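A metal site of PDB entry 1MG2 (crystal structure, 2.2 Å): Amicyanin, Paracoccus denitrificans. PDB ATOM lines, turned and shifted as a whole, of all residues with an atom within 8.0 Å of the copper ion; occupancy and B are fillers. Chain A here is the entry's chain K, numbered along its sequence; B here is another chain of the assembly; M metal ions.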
ATOM      1  N   ILE A  25       7.123  20.784  23.129  1.00  0.00           N
ATOM      2  CA  ILE A  25       5.915  20.072  22.725  1.00  0.00           C
ATOM      3  C   ILE A  25       5.661  20.422  21.265  1.00  0.00           C
ATOM      4  O   ILE A  25       5.586  21.591  20.898  1.00  0.00           O
ATOM      5  CB  ILE A  25       4.693  20.479  23.566  1.00  0.00           C
ATOM      6  CG1 ILE A  25       4.989  20.286  25.055  1.00  0.00           C
ATOM      7  CG2 ILE A  25       3.486  19.602  23.200  1.00  0.00           C
ATOM      8  CD1 ILE A  25       3.918  20.841  25.967  1.00  0.00           C
ATOM      9  N   MET A  28       2.064  16.874  18.277  1.00  0.00           N
ATOM     10  CA  MET A  28       1.231  16.145  19.222  1.00  0.00           C
ATOM     11  C   MET A  28       2.038  15.238  20.156  1.00  0.00           C
ATOM     12  O   MET A  28       1.682  14.077  20.368  1.00  0.00           O
ATOM     13  CB  MET A  28       0.197  15.311  18.464  1.00  0.00           C
ATOM     14  CG  MET A  28      -0.707  16.112  17.531  1.00  0.00           C
ATOM     15  SD  MET A  28      -1.736  17.347  18.368  1.00  0.00           S
ATOM     16  CE  MET A  28      -2.998  16.274  19.093  1.00  0.00           C
ATOM     17  N   LYS A  29       3.135  15.751  20.713  1.00  0.00           N
ATOM     18  CA  LYS A  29       3.934  14.938  21.615  1.00  0.00           C
ATOM     19  C   LYS A  29       4.907  15.734  22.473  1.00  0.00           C
ATOM     20  O   LYS A  29       5.270  16.866  22.141  1.00  0.00           O
ATOM     21  CB  LYS A  29       4.739  13.892  20.828  1.00  0.00           C
ATOM     22  CG  LYS A  29       5.877  14.487  20.011  1.00  0.00           C
ATOM     23  CD  LYS A  29       6.966  13.465  19.699  1.00  0.00           C
ATOM     24  CE  LYS A  29       6.562  12.483  18.608  1.00  0.00           C
ATOM     25  NZ  LYS A  29       6.381  13.143  17.280  1.00  0.00           N
ATOM     26  N   TYR A  30       5.320  15.148  23.591  1.00  0.00           N
ATOM     27  CA  TYR A  30       6.328  15.762  24.448  1.00  0.00           C
ATOM     28  C   TYR A  30       7.597  15.185  23.839  1.00  0.00           C
ATOM     29  O   TYR A  30       7.838  13.991  23.921  1.00  0.00           O
ATOM     30  CB  TYR A  30       6.161  15.279  25.898  1.00  0.00           C
ATOM     31  CG  TYR A  30       4.845  15.697  26.519  1.00  0.00           C
ATOM     32  CD1 TYR A  30       4.572  17.043  26.781  1.00  0.00           C
ATOM     33  CD2 TYR A  30       3.884  14.754  26.853  1.00  0.00           C
ATOM     34  CE1 TYR A  30       3.361  17.426  27.370  1.00  0.00           C
ATOM     35  CE2 TYR A  30       2.674  15.123  27.441  1.00  0.00           C
ATOM     36  CZ  TYR A  30       2.417  16.464  27.690  1.00  0.00           C
ATOM     37  OH  TYR A  30       1.237  16.834  28.293  1.00  0.00           O
ATOM     38  N   ASN A  47       5.194  25.008  24.334  1.00  0.00           N
ATOM     39  CA  ASN A  47       4.419  24.514  23.203  1.00  0.00           C
ATOM     40  C   ASN A  47       4.907  25.201  21.944  1.00  0.00           C
ATOM     41  O   ASN A  47       4.859  26.423  21.836  1.00  0.00           O
ATOM     42  CB  ASN A  47       2.939  24.798  23.418  1.00  0.00           C
ATOM     43  CG  ASN A  47       2.072  24.226  22.322  1.00  0.00           C
ATOM     44  OD1 ASN A  47       2.575  23.637  21.351  1.00  0.00           O
ATOM     45  ND2 ASN A  47       0.754  24.375  22.461  1.00  0.00           N
ATOM     46  N   GLU A  49       3.634  24.581  18.871  1.00  0.00           N
ATOM     47  CA  GLU A  49       2.626  24.579  17.807  1.00  0.00           C
ATOM     48  C   GLU A  49       1.319  25.271  18.190  1.00  0.00           C
ATOM     49  O   GLU A  49       1.092  25.621  19.352  1.00  0.00           O
ATOM     50  CB  GLU A  49       2.356  23.130  17.339  1.00  0.00           C
ATOM     51  CG  GLU A  49       1.799  22.186  18.398  1.00  0.00           C
ATOM     52  CD  GLU A  49       1.514  20.797  17.827  1.00  0.00           C
ATOM     53  OE1 GLU A  49       1.238  20.722  16.603  1.00  0.00           O
ATOM     54  OE2 GLU A  49       1.547  19.799  18.584  1.00  0.00           O
ATOM     55  N   MET A  51      -1.666  23.991  18.077  1.00  0.00           N
ATOM     56  CA  MET A  51      -2.490  23.065  18.837  1.00  0.00           C
ATOM     57  C   MET A  51      -2.197  23.283  20.328  1.00  0.00           C
ATOM     58  O   MET A  51      -1.075  23.080  20.779  1.00  0.00           O
ATOM     59  CB  MET A  51      -2.134  21.622  18.472  1.00  0.00           C
ATOM     60  CG  MET A  51      -2.920  20.577  19.254  1.00  0.00           C
ATOM     61  SD  MET A  51      -4.707  20.632  18.949  1.00  0.00           S
ATOM     62  CE  MET A  51      -4.780  19.873  17.312  1.00  0.00           C
ATOM     63  N   PRO A  52      -3.206  23.729  21.088  1.00  0.00           N
ATOM     64  CA  PRO A  52      -2.951  23.941  22.519  1.00  0.00           C
ATOM     65  C   PRO A  52      -2.656  22.628  23.236  1.00  0.00           C
ATOM     66  O   PRO A  52      -3.239  21.576  22.925  1.00  0.00           O
ATOM     67  CB  PRO A  52      -4.260  24.571  23.006  1.00  0.00           C
ATOM     68  CG  PRO A  52      -4.839  25.201  21.765  1.00  0.00           C
ATOM     69  CD  PRO A  52      -4.559  24.155  20.718  1.00  0.00           C
ATOM     70  N   HIS A  53      -1.744  22.692  24.197  1.00  0.00           N
ATOM     71  CA  HIS A  53      -1.350  21.537  25.013  1.00  0.00           C
ATOM     72  C   HIS A  53      -1.110  22.040  26.429  1.00  0.00           C
ATOM     73  O   HIS A  53      -0.941  23.239  26.647  1.00  0.00           O
ATOM     74  CB  HIS A  53      -0.026  20.930  24.514  1.00  0.00           C
ATOM     75  CG  HIS A  53      -0.064  20.440  23.104  1.00  0.00           C
ATOM     76  ND1 HIS A  53      -0.767  19.337  22.671  1.00  0.00           N
ATOM     77  CD2 HIS A  53       0.592  20.903  22.006  1.00  0.00           C
ATOM     78  CE1 HIS A  53      -0.520  19.173  21.364  1.00  0.00           C
ATOM     79  NE2 HIS A  53       0.298  20.098  20.915  1.00  0.00           N
ATOM     80  N   ASN A  54      -1.071  21.124  27.398  1.00  0.00           N
ATOM     81  CA  ASN A  54      -0.776  21.483  28.785  1.00  0.00           C
ATOM     82  C   ASN A  54      -0.087  20.258  29.392  1.00  0.00           C
ATOM     83  O   ASN A  54       0.296  19.337  28.684  1.00  0.00           O
ATOM     84  CB  ASN A  54      -2.077  21.796  29.548  1.00  0.00           C
ATOM     85  CG  ASN A  54      -2.853  20.549  29.940  1.00  0.00           C
ATOM     86  OD1 ASN A  54      -2.835  19.541  29.228  1.00  0.00           O
ATOM     87  ND2 ASN A  54      -3.549  20.615  31.067  1.00  0.00           N
ATOM     88  N   VAL A  55       0.093  20.272  30.705  1.00  0.00           N
ATOM     89  CA  VAL A  55       0.683  19.135  31.404  1.00  0.00           C
ATOM     90  C   VAL A  55      -0.333  18.841  32.493  1.00  0.00           C
ATOM     91  O   VAL A  55      -0.836  19.765  33.130  1.00  0.00           O
ATOM     92  CB  VAL A  55       2.067  19.467  32.002  1.00  0.00           C
ATOM     93  CG1 VAL A  55       3.097  19.522  30.877  1.00  0.00           C
ATOM     94  CG2 VAL A  55       2.026  20.783  32.769  1.00  0.00           C
ATOM     95  N   MET A  71      -3.696  25.555  29.577  1.00  0.00           N
ATOM     96  CA  MET A  71      -3.347  25.195  28.204  1.00  0.00           C
ATOM     97  C   MET A  71      -2.398  26.247  27.662  1.00  0.00           C
ATOM     98  O   MET A  71      -2.620  27.445  27.833  1.00  0.00           O
ATOM     99  CB  MET A  71      -4.601  25.127  27.323  1.00  0.00           C
ATOM    100  CG  MET A  71      -5.639  24.103  27.756  1.00  0.00           C
ATOM    101  SD  MET A  71      -4.980  22.428  27.777  1.00  0.00           S
ATOM    102  CE  MET A  71      -4.948  22.093  26.029  1.00  0.00           C
ATOM    103  N   MET A  72      -1.331  25.800  27.021  1.00  0.00           N
ATOM    104  CA  MET A  72      -0.347  26.707  26.427  1.00  0.00           C
ATOM    105  C   MET A  72      -0.641  26.857  24.936  1.00  0.00           C
ATOM    106  O   MET A  72      -0.925  25.878  24.247  1.00  0.00           O
ATOM    107  CB  MET A  72       1.067  26.153  26.584  1.00  0.00           C
ATOM    108  CG  MET A  72       1.612  26.087  28.003  1.00  0.00           C
ATOM    109  SD  MET A  72       3.096  25.044  28.094  1.00  0.00           S
ATOM    110  CE  MET A  72       2.322  23.393  28.346  1.00  0.00           C
ATOM    111  N   HIS A  91       0.131  13.903  31.496  1.00  0.00           N
ATOM    112  CA  HIS A  91      -0.395  13.747  30.153  1.00  0.00           C
ATOM    113  C   HIS A  91      -1.044  15.064  29.768  1.00  0.00           C
ATOM    114  O   HIS A  91      -1.108  15.986  30.580  1.00  0.00           O
ATOM    115  CB  HIS A  91      -1.436  12.633  30.090  1.00  0.00           C
ATOM    116  CG  HIS A  91      -2.700  12.964  30.811  1.00  0.00           C
ATOM    117  ND1 HIS A  91      -2.805  12.964  32.185  1.00  0.00           N
ATOM    118  CD2 HIS A  91      -3.911  13.361  30.341  1.00  0.00           C
ATOM    119  CE1 HIS A  91      -4.023  13.344  32.537  1.00  0.00           C
ATOM    120  NE2 HIS A  91      -4.714  13.599  31.437  1.00  0.00           N
ATOM    121  N   CYS A  92      -1.528  15.154  28.543  1.00  0.00           N
ATOM    122  CA  CYS A  92      -2.190  16.366  28.092  1.00  0.00           C
ATOM    123  C   CYS A  92      -3.676  16.092  28.239  1.00  0.00           C
ATOM    124  O   CYS A  92      -4.200  15.135  27.663  1.00  0.00           O
ATOM    125  CB  CYS A  92      -1.826  16.663  26.640  1.00  0.00           C
ATOM    126  SG  CYS A  92      -2.564  18.190  26.044  1.00  0.00           S
ATOM    127  N   THR A  93      -4.366  16.949  28.987  1.00  0.00           N
ATOM    128  CA  THR A  93      -5.776  16.767  29.252  1.00  0.00           C
ATOM    129  C   THR A  93      -6.639  16.385  28.049  1.00  0.00           C
ATOM    130  O   THR A  93      -7.198  15.279  28.013  1.00  0.00           O
ATOM    131  CB  THR A  93      -6.361  18.009  29.941  1.00  0.00           C
ATOM    132  OG1 THR A  93      -5.635  18.262  31.150  1.00  0.00           O
ATOM    133  CG2 THR A  93      -7.833  17.776  30.306  1.00  0.00           C
ATOM    134  N   PRO A  94      -6.735  17.249  27.036  1.00  0.00           N
ATOM    135  CA  PRO A  94      -7.563  16.902  25.869  1.00  0.00           C
ATOM    136  C   PRO A  94      -6.985  15.789  24.994  1.00  0.00           C
ATOM    137  O   PRO A  94      -7.692  15.214  24.167  1.00  0.00           O
ATOM    138  CB  PRO A  94      -7.675  18.227  25.134  1.00  0.00           C
ATOM    139  CG  PRO A  94      -6.317  18.836  25.382  1.00  0.00           C
ATOM    140  CD  PRO A  94      -6.110  18.575  26.853  1.00  0.00           C
ATOM    141  N   HIS A  95      -5.708  15.487  25.182  1.00  0.00           N
ATOM    142  CA  HIS A  95      -5.022  14.462  24.387  1.00  0.00           C
ATOM    143  C   HIS A  95      -4.346  13.441  25.311  1.00  0.00           C
ATOM    144  O   HIS A  95      -3.122  13.476  25.500  1.00  0.00           O
ATOM    145  CB  HIS A  95      -3.981  15.139  23.480  1.00  0.00           C
ATOM    146  CG  HIS A  95      -4.490  16.373  22.793  1.00  0.00           C
ATOM    147  ND1 HIS A  95      -3.774  17.538  22.692  1.00  0.00           N
ATOM    148  CD2 HIS A  95      -5.680  16.601  22.179  1.00  0.00           C
ATOM    149  CE1 HIS A  95      -4.536  18.434  22.041  1.00  0.00           C
ATOM    150  NE2 HIS A  95      -5.701  17.913  21.705  1.00  0.00           N
ATOM    151  N   PRO A  96      -5.134  12.539  25.915  1.00  0.00           N
ATOM    152  CA  PRO A  96      -4.626  11.507  26.831  1.00  0.00           C
ATOM    153  C   PRO A  96      -3.550  10.612  26.224  1.00  0.00           C
ATOM    154  O   PRO A  96      -2.806   9.967  26.952  1.00  0.00           O
ATOM    155  CB  PRO A  96      -5.886  10.734  27.210  1.00  0.00           C
ATOM    156  CG  PRO A  96      -6.959  11.756  27.074  1.00  0.00           C
ATOM    157  CD  PRO A  96      -6.600  12.435  25.789  1.00  0.00           C
ATOM    158  N   PHE A  97      -3.474  10.566  24.900  1.00  0.00           N
ATOM    159  CA  PHE A  97      -2.457   9.740  24.249  1.00  0.00           C
ATOM    160  C   PHE A  97      -1.074  10.384  24.374  1.00  0.00           C
ATOM    161  O   PHE A  97      -0.053   9.739  24.116  1.00  0.00           O
ATOM    162  CB  PHE A  97      -2.801   9.524  22.774  1.00  0.00           C
ATOM    163  CG  PHE A  97      -3.066  10.784  22.020  1.00  0.00           C
ATOM    164  CD1 PHE A  97      -4.345  11.347  21.999  1.00  0.00           C
ATOM    165  CD2 PHE A  97      -2.039  11.435  21.343  1.00  0.00           C
ATOM    166  CE1 PHE A  97      -4.595  12.527  21.311  1.00  0.00           C
ATOM    167  CE2 PHE A  97      -2.267  12.623  20.650  1.00  0.00           C
ATOM    168  CZ  PHE A  97      -3.551  13.165  20.632  1.00  0.00           C
ATOM    169  N   MET A  98      -1.041  11.667  24.750  1.00  0.00           N
ATOM    170  CA  MET A  98       0.219  12.385  24.934  1.00  0.00           C
ATOM    171  C   MET A  98       0.682  12.171  26.368  1.00  0.00           C
ATOM    172  O   MET A  98       0.084  12.691  27.313  1.00  0.00           O
ATOM    173  CB  MET A  98       0.039  13.890  24.674  1.00  0.00           C
ATOM    174  CG  MET A  98      -0.083  14.276  23.224  1.00  0.00           C
ATOM    175  SD  MET A  98      -0.335  16.043  23.020  1.00  0.00           S
ATOM    176  CE  MET A  98       1.296  16.656  23.395  1.00  0.00           C
ATOM    177  N   GLU B 101      -8.344  15.259  19.270  1.00  0.00           N
ATOM    178  CA  GLU B 101      -7.966  16.660  19.116  1.00  0.00           C
ATOM    179  C   GLU B 101      -8.863  17.400  18.127  1.00  0.00           C
ATOM    180  O   GLU B 101      -8.977  18.631  18.199  1.00  0.00           O
ATOM    181  CB  GLU B 101      -6.497  16.790  18.677  1.00  0.00           C
ATOM    182  CG  GLU B 101      -6.183  16.186  17.320  1.00  0.00           C
ATOM    183  CD  GLU B 101      -5.789  14.724  17.410  1.00  0.00           C
ATOM    184  OE1 GLU B 101      -6.272  14.019  18.320  1.00  0.00           O
ATOM    185  OE2 GLU B 101      -5.001  14.277  16.543  1.00  0.00           O
HETATM  186 CU    CU M   1      -2.008  18.104  23.790  1.00  0.00          CU
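The copper ion is bound by a ring nitrogen (ND1) of His 53 (2.1 Å), a ring nitrogen (ND1) of His 95 (2.2 Å), the side-chain sulfur of Cys 92 (2.3 Å) and the side-chain sulfur of Met 98 (2.8 Å).
Pro 52 touches the copper ion.
NE2 of His 53 lies close to O of Met 51 (3.3 Å).
A ring nitrogen (NE2) of His 53 lies within hydrogen-bond range of the side-chain carboxylate (OE2) of Glu 49, at 2.7 Å.
The backbone NH of His 53 lies close to the side-chain amide nitrogen of Asn 47.
O of His 53 is in hydrogen-bond range of N of Met 72 (2.6 Å).
The side-chain amide oxygen (OD1) of Asn 54 lies close to the side-chain sulfur (SG) of Cys 92 (3.5 Å).
N of Cys 92 sits at hydrogen-bond distance from OH of Tyr 30, 3.2 Å away.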
